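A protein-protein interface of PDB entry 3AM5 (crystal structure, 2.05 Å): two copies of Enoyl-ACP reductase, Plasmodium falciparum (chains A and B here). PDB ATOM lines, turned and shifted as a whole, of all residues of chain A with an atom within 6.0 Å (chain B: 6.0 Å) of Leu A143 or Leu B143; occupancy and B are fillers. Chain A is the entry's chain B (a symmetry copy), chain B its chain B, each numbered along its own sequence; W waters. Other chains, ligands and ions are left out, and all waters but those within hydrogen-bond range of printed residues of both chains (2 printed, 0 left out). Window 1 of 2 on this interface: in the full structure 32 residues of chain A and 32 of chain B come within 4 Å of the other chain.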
ATOM      1  N   ASN A 123     -18.241  -2.344 -17.336  1.00  0.00           N
ATOM      2  CA  ASN A 123     -19.289  -1.645 -18.038  1.00  0.00           C
ATOM      3  C   ASN A 123     -20.195  -0.912 -17.059  1.00  0.00           C
ATOM      4  O   ASN A 123     -20.315  -1.307 -15.876  1.00  0.00           O
ATOM      5  CB  ASN A 123     -20.068  -2.579 -18.969  1.00  0.00           C
ATOM      6  CG  ASN A 123     -20.119  -2.024 -20.385  1.00  0.00           C
ATOM      7  OD1 ASN A 123     -20.078  -2.773 -21.367  1.00  0.00           O
ATOM      8  ND2 ASN A 123     -20.153  -0.686 -20.494  1.00  0.00           N
ATOM      9  N   ARG A 136     -30.606   4.654  -9.941  1.00  0.00           N
ATOM     10  CA  ARG A 136     -30.449   3.372  -9.267  1.00  0.00           C
ATOM     11  C   ARG A 136     -30.080   2.283 -10.283  1.00  0.00           C
ATOM     12  O   ARG A 136     -29.168   1.486 -10.059  1.00  0.00           O
ATOM     13  CB  ARG A 136     -31.719   2.991  -8.518  1.00  0.00           C
ATOM     14  CG  ARG A 136     -31.599   1.720  -7.651  1.00  0.00           C
ATOM     15  CD  ARG A 136     -32.865   1.503  -6.801  1.00  0.00           C
ATOM     16  NE  ARG A 136     -33.113   2.617  -5.870  1.00  0.00           N
ATOM     17  CZ  ARG A 136     -32.821   2.639  -4.568  1.00  0.00           C
ATOM     18  NH1 ARG A 136     -32.230   1.599  -3.974  1.00  0.00           N
ATOM     19  NH2 ARG A 136     -33.126   3.722  -3.846  1.00  0.00           N
ATOM     20  N   GLY A 138     -28.726   2.587 -13.337  1.00  0.00           N
ATOM     21  CA  GLY A 138     -27.375   2.787 -13.886  1.00  0.00           C
ATOM     22  C   GLY A 138     -26.299   2.296 -12.889  1.00  0.00           C
ATOM     23  O   GLY A 138     -25.377   1.579 -13.264  1.00  0.00           O
ATOM     24  N   TYR A 139     -26.454   2.652 -11.613  1.00  0.00           N
ATOM     25  CA  TYR A 139     -25.499   2.225 -10.571  1.00  0.00           C
ATOM     26  C   TYR A 139     -25.441   0.699 -10.447  1.00  0.00           C
ATOM     27  O   TYR A 139     -24.363   0.091 -10.404  1.00  0.00           O
ATOM     28  CB  TYR A 139     -25.982   2.785  -9.254  1.00  0.00           C
ATOM     29  CG  TYR A 139     -25.087   2.624  -8.044  1.00  0.00           C
ATOM     30  CD1 TYR A 139     -25.320   1.609  -7.114  1.00  0.00           C
ATOM     31  CD2 TYR A 139     -24.067   3.558  -7.779  1.00  0.00           C
ATOM     32  CE1 TYR A 139     -24.524   1.494  -5.960  1.00  0.00           C
ATOM     33  CE2 TYR A 139     -23.286   3.466  -6.625  1.00  0.00           C
ATOM     34  CZ  TYR A 139     -23.521   2.423  -5.719  1.00  0.00           C
ATOM     35  OH  TYR A 139     -22.777   2.335  -4.559  1.00  0.00           O
ATOM     36  N   LEU A 140     -26.612   0.080 -10.369  1.00  0.00           N
ATOM     37  CA  LEU A 140     -26.656  -1.374 -10.253  1.00  0.00           C
ATOM     38  C   LEU A 140     -26.114  -2.050 -11.493  1.00  0.00           C
ATOM     39  O   LEU A 140     -25.522  -3.117 -11.394  1.00  0.00           O
ATOM     40  CB  LEU A 140     -28.069  -1.865  -9.909  1.00  0.00           C
ATOM     41  CG  LEU A 140     -28.594  -1.380  -8.543  1.00  0.00           C
ATOM     42  CD1 LEU A 140     -30.046  -1.856  -8.356  1.00  0.00           C
ATOM     43  CD2 LEU A 140     -27.716  -1.862  -7.370  1.00  0.00           C
ATOM     44  N   ASP A 141     -26.291  -1.422 -12.663  1.00  0.00           N
ATOM     45  CA  ASP A 141     -25.689  -1.939 -13.881  1.00  0.00           C
ATOM     46  C   ASP A 141     -24.162  -1.951 -13.740  1.00  0.00           C
ATOM     47  O   ASP A 141     -23.511  -2.947 -14.052  1.00  0.00           O
ATOM     48  CB  ASP A 141     -26.079  -1.074 -15.085  1.00  0.00           C
ATOM     49  CG  ASP A 141     -25.505  -1.605 -16.379  1.00  0.00           C
ATOM     50  OD1 ASP A 141     -24.604  -0.965 -16.967  1.00  0.00           O
ATOM     51  OD2 ASP A 141     -25.937  -2.694 -16.788  1.00  0.00           O
ATOM     52  N   ALA A 142     -23.591  -0.846 -13.257  1.00  0.00           N
ATOM     53  CA  ALA A 142     -22.130  -0.752 -13.130  1.00  0.00           C
ATOM     54  C   ALA A 142     -21.611  -1.859 -12.164  1.00  0.00           C
ATOM     55  O   ALA A 142     -20.658  -2.544 -12.469  1.00  0.00           O
ATOM     56  CB  ALA A 142     -21.744   0.629 -12.613  1.00  0.00           C
ATOM     57  N   LEU A 143     -22.300  -2.051 -11.038  1.00  0.00           N
ATOM     58  CA  LEU A 143     -21.898  -3.076 -10.054  1.00  0.00           C
ATOM     59  C   LEU A 143     -22.064  -4.482 -10.607  1.00  0.00           C
ATOM     60  O   LEU A 143     -21.207  -5.335 -10.412  1.00  0.00           O
ATOM     61  CB  LEU A 143     -22.679  -2.924  -8.737  1.00  0.00           C
ATOM     62  CG  LEU A 143     -22.109  -1.931  -7.710  1.00  0.00           C
ATOM     63  CD1 LEU A 143     -20.843  -2.496  -7.011  1.00  0.00           C
ATOM     64  CD2 LEU A 143     -21.801  -0.549  -8.320  1.00  0.00           C
ATOM     65  N   SER A 144     -23.197  -4.711 -11.273  1.00  0.00           N
ATOM     66  CA  SER A 144     -23.481  -6.010 -11.866  1.00  0.00           C
ATOM     67  C   SER A 144     -22.405  -6.443 -12.854  1.00  0.00           C
ATOM     68  O   SER A 144     -21.844  -7.549 -12.777  1.00  0.00           O
ATOM     69  CB  SER A 144     -24.833  -5.993 -12.587  1.00  0.00           C
ATOM     70  OG  SER A 144     -25.101  -7.320 -13.052  1.00  0.00           O
ATOM     71  N   LYS A 145     -22.112  -5.553 -13.794  1.00  0.00           N
ATOM     72  CA  LYS A 145     -21.212  -5.904 -14.879  1.00  0.00           C
ATOM     73  C   LYS A 145     -19.740  -5.804 -14.494  1.00  0.00           C
ATOM     74  O   LYS A 145     -18.916  -6.583 -14.978  1.00  0.00           O
ATOM     75  CB  LYS A 145     -21.519  -5.058 -16.117  1.00  0.00           C
ATOM     76  CG  LYS A 145     -22.712  -5.599 -16.914  1.00  0.00           C
ATOM     77  CD  LYS A 145     -23.321  -4.564 -17.824  1.00  0.00           C
ATOM     78  CE  LYS A 145     -24.617  -5.081 -18.458  1.00  0.00           C
ATOM     79  NZ  LYS A 145     -25.403  -3.988 -19.092  1.00  0.00           N
ATOM     80  N   SER A 146     -19.403  -4.867 -13.618  1.00  0.00           N
ATOM     81  CA  SER A 146     -17.975  -4.611 -13.329  1.00  0.00           C
ATOM     82  C   SER A 146     -17.440  -5.305 -12.081  1.00  0.00           C
ATOM     83  O   SER A 146     -16.236  -5.485 -11.969  1.00  0.00           O
ATOM     84  CB  SER A 146     -17.710  -3.120 -13.155  1.00  0.00           C
ATOM     85  OG  SER A 146     -18.212  -2.391 -14.262  1.00  0.00           O
ATOM     86  N   SER A 147     -18.324  -5.638 -11.145  1.00  0.00           N
ATOM     87  CA  SER A 147     -17.881  -6.140  -9.820  1.00  0.00           C
ATOM     88  C   SER A 147     -18.446  -7.530  -9.609  1.00  0.00           C
ATOM     89  O   SER A 147     -17.678  -8.454  -9.360  1.00  0.00           O
ATOM     90  CB  SER A 147     -18.337  -5.210  -8.694  1.00  0.00           C
ATOM     91  OG  SER A 147     -18.038  -3.856  -9.036  1.00  0.00           O
ATOM     92  N   TYR A 148     -19.776  -7.688  -9.708  1.00  0.00           N
ATOM     93  CA  TYR A 148     -20.363  -8.998  -9.427  1.00  0.00           C
ATOM     94  C   TYR A 148     -19.850 -10.050 -10.405  1.00  0.00           C
ATOM     95  O   TYR A 148     -19.664 -11.213 -10.047  1.00  0.00           O
ATOM     96  CB  TYR A 148     -21.924  -9.012  -9.365  1.00  0.00           C
ATOM     97  CG  TYR A 148     -22.386 -10.413  -9.015  1.00  0.00           C
ATOM     98  CD1 TYR A 148     -22.337 -10.871  -7.700  1.00  0.00           C
ATOM     99  CD2 TYR A 148     -22.730 -11.316 -10.017  1.00  0.00           C
ATOM    100  CE1 TYR A 148     -22.648 -12.189  -7.388  1.00  0.00           C
ATOM    101  CE2 TYR A 148     -23.069 -12.637  -9.722  1.00  0.00           C
ATOM    102  CZ  TYR A 148     -23.019 -13.069  -8.410  1.00  0.00           C
ATOM    103  OH  TYR A 148     -23.358 -14.373  -8.119  1.00  0.00           O
ATOM    104  N   SER A 149     -19.642  -9.650 -11.652  1.00  0.00           N
ATOM    105  CA  SER A 149     -19.093 -10.551 -12.658  1.00  0.00           C
ATOM    106  C   SER A 149     -17.787 -11.268 -12.224  1.00  0.00           C
ATOM    107  O   SER A 149     -17.544 -12.401 -12.630  1.00  0.00           O
ATOM    108  CB  SER A 149     -18.837  -9.797 -13.954  1.00  0.00           C
ATOM    109  OG  SER A 149     -17.932  -8.735 -13.744  1.00  0.00           O
ATOM    110  N   GLY A 185     -21.191   5.323 -11.222  1.00  0.00           N
ATOM    111  CA  GLY A 185     -20.954   4.244 -10.250  1.00  0.00           C
ATOM    112  C   GLY A 185     -19.761   3.349 -10.614  1.00  0.00           C
ATOM    113  O   GLY A 185     -19.546   2.335  -9.961  1.00  0.00           O
ATOM    114  N   SER A 188     -17.652   3.319  -7.564  1.00  0.00           N
ATOM    115  CA  SER A 188     -18.305   2.444  -6.567  1.00  0.00           C
ATOM    116  C   SER A 188     -18.007   0.986  -6.902  1.00  0.00           C
ATOM    117  O   SER A 188     -17.652   0.192  -6.035  1.00  0.00           O
ATOM    118  CB  SER A 188     -19.817   2.698  -6.619  1.00  0.00           C
ATOM    119  OG  SER A 188     -20.046   4.102  -6.834  1.00  0.00           O
ATOM    120  N   ALA A 189     -18.194   0.644  -8.163  1.00  0.00           N
ATOM    121  CA  ALA A 189     -17.862  -0.688  -8.660  1.00  0.00           C
ATOM    122  C   ALA A 189     -16.396  -1.095  -8.410  1.00  0.00           C
ATOM    123  O   ALA A 189     -16.132  -2.249  -8.059  1.00  0.00           O
ATOM    124  CB  ALA A 189     -18.189  -0.781 -10.136  1.00  0.00           C
ATOM    125  N   ALA A 192     -15.907  -1.750  -4.662  1.00  0.00           N
ATOM    126  CA  ALA A 192     -16.476  -3.075  -4.391  1.00  0.00           C
ATOM    127  C   ALA A 192     -15.534  -4.204  -4.848  1.00  0.00           C
ATOM    128  O   ALA A 192     -15.249  -5.131  -4.087  1.00  0.00           O
ATOM    129  CB  ALA A 192     -17.828  -3.206  -5.065  1.00  0.00           C
ATOM    130  N   ASN B 123     -29.506  -3.264   4.223  1.00  0.00           N
ATOM    131  CA  ASN B 123     -30.216  -4.497   3.983  1.00  0.00           C
ATOM    132  C   ASN B 123     -29.541  -5.299   2.881  1.00  0.00           C
ATOM    133  O   ASN B 123     -28.850  -4.732   2.004  1.00  0.00           O
ATOM    134  CB  ASN B 123     -31.701  -4.250   3.702  1.00  0.00           C
ATOM    135  CG  ASN B 123     -32.579  -5.087   4.621  1.00  0.00           C
ATOM    136  OD1 ASN B 123     -33.654  -4.652   5.049  1.00  0.00           O
ATOM    137  ND2 ASN B 123     -32.090  -6.287   4.973  1.00  0.00           N
ATOM    138  N   ARG B 136     -26.251 -13.028  -8.050  1.00  0.00           N
ATOM    139  CA  ARG B 136     -26.222 -11.689  -8.625  1.00  0.00           C
ATOM    140  C   ARG B 136     -27.324 -10.823  -8.001  1.00  0.00           C
ATOM    141  O   ARG B 136     -27.090  -9.678  -7.612  1.00  0.00           O
ATOM    142  CB  ARG B 136     -26.380 -11.742 -10.138  1.00  0.00           C
ATOM    143  CG  ARG B 136     -26.211 -10.383 -10.851  1.00  0.00           C
ATOM    144  CD  ARG B 136     -26.217 -10.552 -12.381  1.00  0.00           C
ATOM    145  NE  ARG B 136     -25.116 -11.406 -12.855  1.00  0.00           N
ATOM    146  CZ  ARG B 136     -23.963 -10.990 -13.385  1.00  0.00           C
ATOM    147  NH1 ARG B 136     -23.693  -9.689 -13.517  1.00  0.00           N
ATOM    148  NH2 ARG B 136     -23.062 -11.892 -13.787  1.00  0.00           N
ATOM    149  N   GLY B 138     -28.952 -11.210  -5.094  1.00  0.00           N
ATOM    150  CA  GLY B 138     -28.682 -10.917  -3.677  1.00  0.00           C
ATOM    151  C   GLY B 138     -27.639  -9.783  -3.539  1.00  0.00           C
ATOM    152  O   GLY B 138     -27.831  -8.844  -2.773  1.00  0.00           O
ATOM    153  N   TYR B 139     -26.561  -9.859  -4.321  1.00  0.00           N
ATOM    154  CA  TYR B 139     -25.510  -8.823  -4.288  1.00  0.00           C
ATOM    155  C   TYR B 139     -26.059  -7.446  -4.676  1.00  0.00           C
ATOM    156  O   TYR B 139     -25.808  -6.434  -4.007  1.00  0.00           O
ATOM    157  CB  TYR B 139     -24.457  -9.211  -5.301  1.00  0.00           C
ATOM    158  CG  TYR B 139     -23.185  -8.392  -5.351  1.00  0.00           C
ATOM    159  CD1 TYR B 139     -23.015  -7.396  -6.314  1.00  0.00           C
ATOM    160  CD2 TYR B 139     -22.109  -8.689  -4.492  1.00  0.00           C
ATOM    161  CE1 TYR B 139     -21.811  -6.673  -6.397  1.00  0.00           C
ATOM    162  CE2 TYR B 139     -20.901  -7.993  -4.582  1.00  0.00           C
ATOM    163  CZ  TYR B 139     -20.763  -6.980  -5.540  1.00  0.00           C
ATOM    164  OH  TYR B 139     -19.566  -6.303  -5.660  1.00  0.00           O
ATOM    165  N   LEU B 140     -26.798  -7.407  -5.777  1.00  0.00           N
ATOM    166  CA  LEU B 140     -27.368  -6.140  -6.222  1.00  0.00           C
ATOM    167  C   LEU B 140     -28.385  -5.608  -5.235  1.00  0.00           C
ATOM    168  O   LEU B 140     -28.511  -4.399  -5.085  1.00  0.00           O
ATOM    169  CB  LEU B 140     -27.954  -6.255  -7.636  1.00  0.00           C
ATOM    170  CG  LEU B 140     -26.916  -6.584  -8.727  1.00  0.00           C
ATOM    171  CD1 LEU B 140     -27.634  -6.768 -10.076  1.00  0.00           C
ATOM    172  CD2 LEU B 140     -25.821  -5.504  -8.844  1.00  0.00           C
ATOM    173  N   ASP B 141     -29.097  -6.505  -4.542  1.00  0.00           N
ATOM    174  CA  ASP B 141     -30.000  -6.080  -3.485  1.00  0.00           C
ATOM    175  C   ASP B 141     -29.208  -5.363  -2.384  1.00  0.00           C
ATOM    176  O   ASP B 141     -29.595  -4.287  -1.931  1.00  0.00           O
ATOM    177  CB  ASP B 141     -30.729  -7.285  -2.880  1.00  0.00           C
ATOM    178  CG  ASP B 141     -31.710  -6.877  -1.804  1.00  0.00           C
ATOM    179  OD1 ASP B 141     -31.478  -7.173  -0.610  1.00  0.00           O
ATOM    180  OD2 ASP B 141     -32.702  -6.220  -2.157  1.00  0.00           O
ATOM    181  N   ALA B 142     -28.088  -5.956  -1.961  1.00  0.00           N
ATOM    182  CA  ALA B 142     -27.290  -5.364  -0.879  1.00  0.00           C
ATOM    183  C   ALA B 142     -26.794  -3.948  -1.302  1.00  0.00           C
ATOM    184  O   ALA B 142     -26.902  -3.007  -0.544  1.00  0.00           O
ATOM    185  CB  ALA B 142     -26.107  -6.269  -0.556  1.00  0.00           C
ATOM    186  N   LEU B 143     -26.314  -3.820  -2.539  1.00  0.00           N
ATOM    187  CA  LEU B 143     -25.820  -2.523  -3.043  1.00  0.00           C
ATOM    188  C   LEU B 143     -26.943  -1.509  -3.181  1.00  0.00           C
ATOM    189  O   LEU B 143     -26.781  -0.346  -2.830  1.00  0.00           O
ATOM    190  CB  LEU B 143     -25.082  -2.688  -4.384  1.00  0.00           C
ATOM    191  CG  LEU B 143     -23.590  -3.055  -4.307  1.00  0.00           C
ATOM    192  CD1 LEU B 143     -22.726  -1.844  -3.864  1.00  0.00           C
ATOM    193  CD2 LEU B 143     -23.317  -4.261  -3.385  1.00  0.00           C
ATOM    194  N   SER B 144     -28.072  -1.966  -3.725  1.00  0.00           N
ATOM    195  CA  SER B 144     -29.232  -1.105  -3.907  1.00  0.00           C
ATOM    196  C   SER B 144     -29.705  -0.489  -2.595  1.00  0.00           C
ATOM    197  O   SER B 144     -29.880   0.734  -2.466  1.00  0.00           O
ATOM    198  CB  SER B 144     -30.393  -1.886  -4.532  1.00  0.00           C
ATOM    199  OG  SER B 144     -31.460  -0.963  -4.781  1.00  0.00           O
ATOM    200  N   LYS B 145     -29.912  -1.353  -1.609  1.00  0.00           N
ATOM    201  CA  LYS B 145     -30.503  -0.909  -0.359  1.00  0.00           C
ATOM    202  C   LYS B 145     -29.497  -0.257   0.583  1.00  0.00           C
ATOM    203  O   LYS B 145     -29.845   0.667   1.322  1.00  0.00           O
ATOM    204  CB  LYS B 145     -31.231  -2.069   0.325  1.00  0.00           C
ATOM    205  CG  LYS B 145     -32.626  -2.313  -0.264  1.00  0.00           C
ATOM    206  CD  LYS B 145     -33.151  -3.692   0.039  1.00  0.00           C
ATOM    207  CE  LYS B 145     -34.455  -3.964  -0.719  1.00  0.00           C
ATOM    208  NZ  LYS B 145     -34.820  -5.407  -0.702  1.00  0.00           N
ATOM    209  N   SER B 146     -28.253  -0.713   0.554  1.00  0.00           N
ATOM    210  CA  SER B 146     -27.272  -0.237   1.554  1.00  0.00           C
ATOM    211  C   SER B 146     -26.368   0.893   1.077  1.00  0.00           C
ATOM    212  O   SER B 146     -25.817   1.605   1.904  1.00  0.00           O
ATOM    213  CB  SER B 146     -26.361  -1.372   2.010  1.00  0.00           C
ATOM    214  OG  SER B 146     -27.126  -2.486   2.439  1.00  0.00           O
ATOM    215  N   SER B 147     -26.185   1.013  -0.234  1.00  0.00           N
ATOM    216  CA  SER B 147     -25.178   1.955  -0.783  1.00  0.00           C
ATOM    217  C   SER B 147     -25.881   2.960  -1.672  1.00  0.00           C
ATOM    218  O   SER B 147     -25.748   4.158  -1.439  1.00  0.00           O
ATOM    219  CB  SER B 147     -24.099   1.214  -1.575  1.00  0.00           C
ATOM    220  OG  SER B 147     -23.634   0.092  -0.824  1.00  0.00           O
ATOM    221  N   TYR B 148     -26.625   2.488  -2.685  1.00  0.00           N
ATOM    222  CA  TYR B 148     -27.248   3.431  -3.613  1.00  0.00           C
ATOM    223  C   TYR B 148     -28.241   4.337  -2.892  1.00  0.00           C
ATOM    224  O   TYR B 148     -28.391   5.512  -3.231  1.00  0.00           O
ATOM    225  CB  TYR B 148     -27.910   2.770  -4.866  1.00  0.00           C
ATOM    226  CG  TYR B 148     -28.463   3.863  -5.759  1.00  0.00           C
ATOM    227  CD1 TYR B 148     -27.622   4.592  -6.597  1.00  0.00           C
ATOM    228  CD2 TYR B 148     -29.794   4.258  -5.654  1.00  0.00           C
ATOM    229  CE1 TYR B 148     -28.099   5.670  -7.331  1.00  0.00           C
ATOM    230  CE2 TYR B 148     -30.299   5.323  -6.401  1.00  0.00           C
ATOM    231  CZ  TYR B 148     -29.448   6.029  -7.230  1.00  0.00           C
ATOM    232  OH  TYR B 148     -29.948   7.078  -7.971  1.00  0.00           O
ATOM    233  N   SER B 149     -28.939   3.788  -1.908  1.00  0.00           N
ATOM    234  CA  SER B 149     -29.870   4.574  -1.107  1.00  0.00           C
ATOM    235  C   SER B 149     -29.260   5.873  -0.515  1.00  0.00           C
ATOM    236  O   SER B 149     -29.965   6.865  -0.356  1.00  0.00           O
ATOM    237  CB  SER B 149     -30.429   3.728   0.027  1.00  0.00           C
ATOM    238  OG  SER B 149     -29.391   3.255   0.858  1.00  0.00           O
ATOM    239  N   GLY B 185     -22.711  -9.764   0.168  1.00  0.00           N
ATOM    240  CA  GLY B 185     -22.324  -8.496  -0.470  1.00  0.00           C
ATOM    241  C   GLY B 185     -22.463  -7.281   0.458  1.00  0.00           C
ATOM    242  O   GLY B 185     -22.306  -6.153   0.004  1.00  0.00           O
ATOM    243  N   SER B 188     -19.157  -5.607   0.308  1.00  0.00           N
ATOM    244  CA  SER B 188     -19.063  -4.902  -0.988  1.00  0.00           C
ATOM    245  C   SER B 188     -19.830  -3.586  -0.905  1.00  0.00           C
ATOM    246  O   SER B 188     -19.347  -2.538  -1.323  1.00  0.00           O
ATOM    247  CB  SER B 188     -19.672  -5.800  -2.072  1.00  0.00           C
ATOM    248  OG  SER B 188     -19.324  -7.167  -1.794  1.00  0.00           O
ATOM    249  N   ALA B 189     -21.045  -3.670  -0.394  1.00  0.00           N
ATOM    250  CA  ALA B 189     -21.868  -2.487  -0.159  1.00  0.00           C
ATOM    251  C   ALA B 189     -21.192  -1.429   0.737  1.00  0.00           C
ATOM    252  O   ALA B 189     -21.309  -0.230   0.465  1.00  0.00           O
ATOM    253  CB  ALA B 189     -23.203  -2.898   0.426  1.00  0.00           C
ATOM    254  N   ALA B 192     -18.350   0.237  -1.227  1.00  0.00           N
ATOM    255  CA  ALA B 192     -18.979   1.198  -2.140  1.00  0.00           C
ATOM    256  C   ALA B 192     -19.406   2.484  -1.407  1.00  0.00           C
ATOM    257  O   ALA B 192     -19.095   3.592  -1.848  1.00  0.00           O
ATOM    258  CB  ALA B 192     -20.169   0.558  -2.827  1.00  0.00           C
HETATM  259  O   HOH W   1     -26.344 -15.355  -9.560  1.00  0.00           O
HETATM  260  O   HOH W   2     -32.845   6.274  -9.681  1.00  0.00           O
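OH of Tyr B148 is in hydrogen-bond range of N of Arg A136, at 3.2 Å. The backbone NH of Arg B136 is in hydrogen-bond range of the side-chain hydroxyl of Tyr A148. The side-chain hydroxyl (OG) of Ser B144 sits at hydrogen-bond distance from the guanidinium group (NH1) of Arg A136. The guanidinium group (NH1) of Arg B136 sits at hydrogen-bond distance from the side-chain hydroxyl (OG) of Ser A144, 2.8 Å away.
The backbone carbonyl oxygen (O) of Ser A144 is in hydrogen-bond range of the backbone NH (N) of Ser A149. The backbone carbonyl oxygen (O) of Leu A143 lies within hydrogen-bond range of the backbone NH (N) of Tyr A148 (2.8 Å). The backbone carbonyl oxygen (O) of Ala A189 is in hydrogen-bond range of the side-chain hydroxyl (OG) of Ser A147, 2.7 Å away. The backbone carbonyl oxygen of Ser B144 sits at hydrogen-bond distance from the backbone NH of Ser B149. The side-chain hydroxyl (OG) of Ser B147 lies within hydrogen-bond range of the backbone carbonyl oxygen (O) of Ala B189 (2.7 Å). The backbone NH (N) of Tyr B148 sits at hydrogen-bond distance from the backbone carbonyl oxygen (O) of Leu B143.
Ser B147 touches Tyr A139. CG of Tyr A139 touches CD1 of Tyr B148, 3.5 Å away. Tyr A139 touches Ala B192 (OH to CB, 3.6 Å). Leu B140 touches Leu A140. CD2 of Leu A140 touches N of Ser B144 (3.7 Å). CD1 of Leu B143 touches CD1 of Leu A143 (3.7 Å). N of Ser A144 touches CD2 of Leu B140, 3.7 Å away. Ser A147 touches Tyr B139 (CB to OH, 3.5 Å). Tyr B139 touches Tyr A148 (CG to CD1, 3.5 Å). OH of Tyr B139 touches CB of Ala A192, 3.6 Å away.
Printed residues of chain B within 4 Å of Leu A143: Leu B143. Of chain A, only Leu A143 comes within 4 Å of Leu B143. Of the printed residues of chain B, Ala A192 touches Tyr B139 (3.6 Å). Printed residues of chain A within 4 Å of Tyr B148: Arg A136 (3.2 Å) and Tyr A139 (3.5 Å). Of the printed residues of chain B, Ser A147 touches Tyr B139 (3.5 Å). Asp B141 touches none of the printed residues of chain A. Ala A189 touches none of the printed residues of chain B.
Hydrophobic or aromatic side chains of chain B within 4 Å of the printed part of chain A: Tyr B139, Leu B140, Leu B143, Tyr B148 and Ala B192. Of the 18 printed residues of chain A, 8 touch a printed residue of chain B. Among the printed residues, 14 pairs touch across the chains.
Arg A136 touches Ser B144, and with the chains exchanged Ser A144 touches Arg B136. Arg A136 touches Tyr B148, and with the chains exchanged Tyr A148 touches Arg B136. Tyr A139 touches Ser B147, and with the chains exchanged Ser A147 touches Tyr B139. Tyr A139 touches Ala B192, and with the chains exchanged Ala A192 touches Tyr B139. Positions printed for both chains: 123, 136, 138, 139, 140, 141, 142, 143, 144, 145, 146, 147, 148, 149, 185, 188, 189 and 192. Of the 14 pairs that touch across the chains among the printed residues, 14 have their exchanged pair printed and touching as well.
Water W2 bridges the backbone NH of Arg A136 (2.8 Å) and the side-chain hydroxyl of Tyr B148 (3.5 Å). Water W1 lies within hydrogen-bond range of N of Arg B136 (2.8 Å) and OH of Tyr A148 (3.5 Å).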
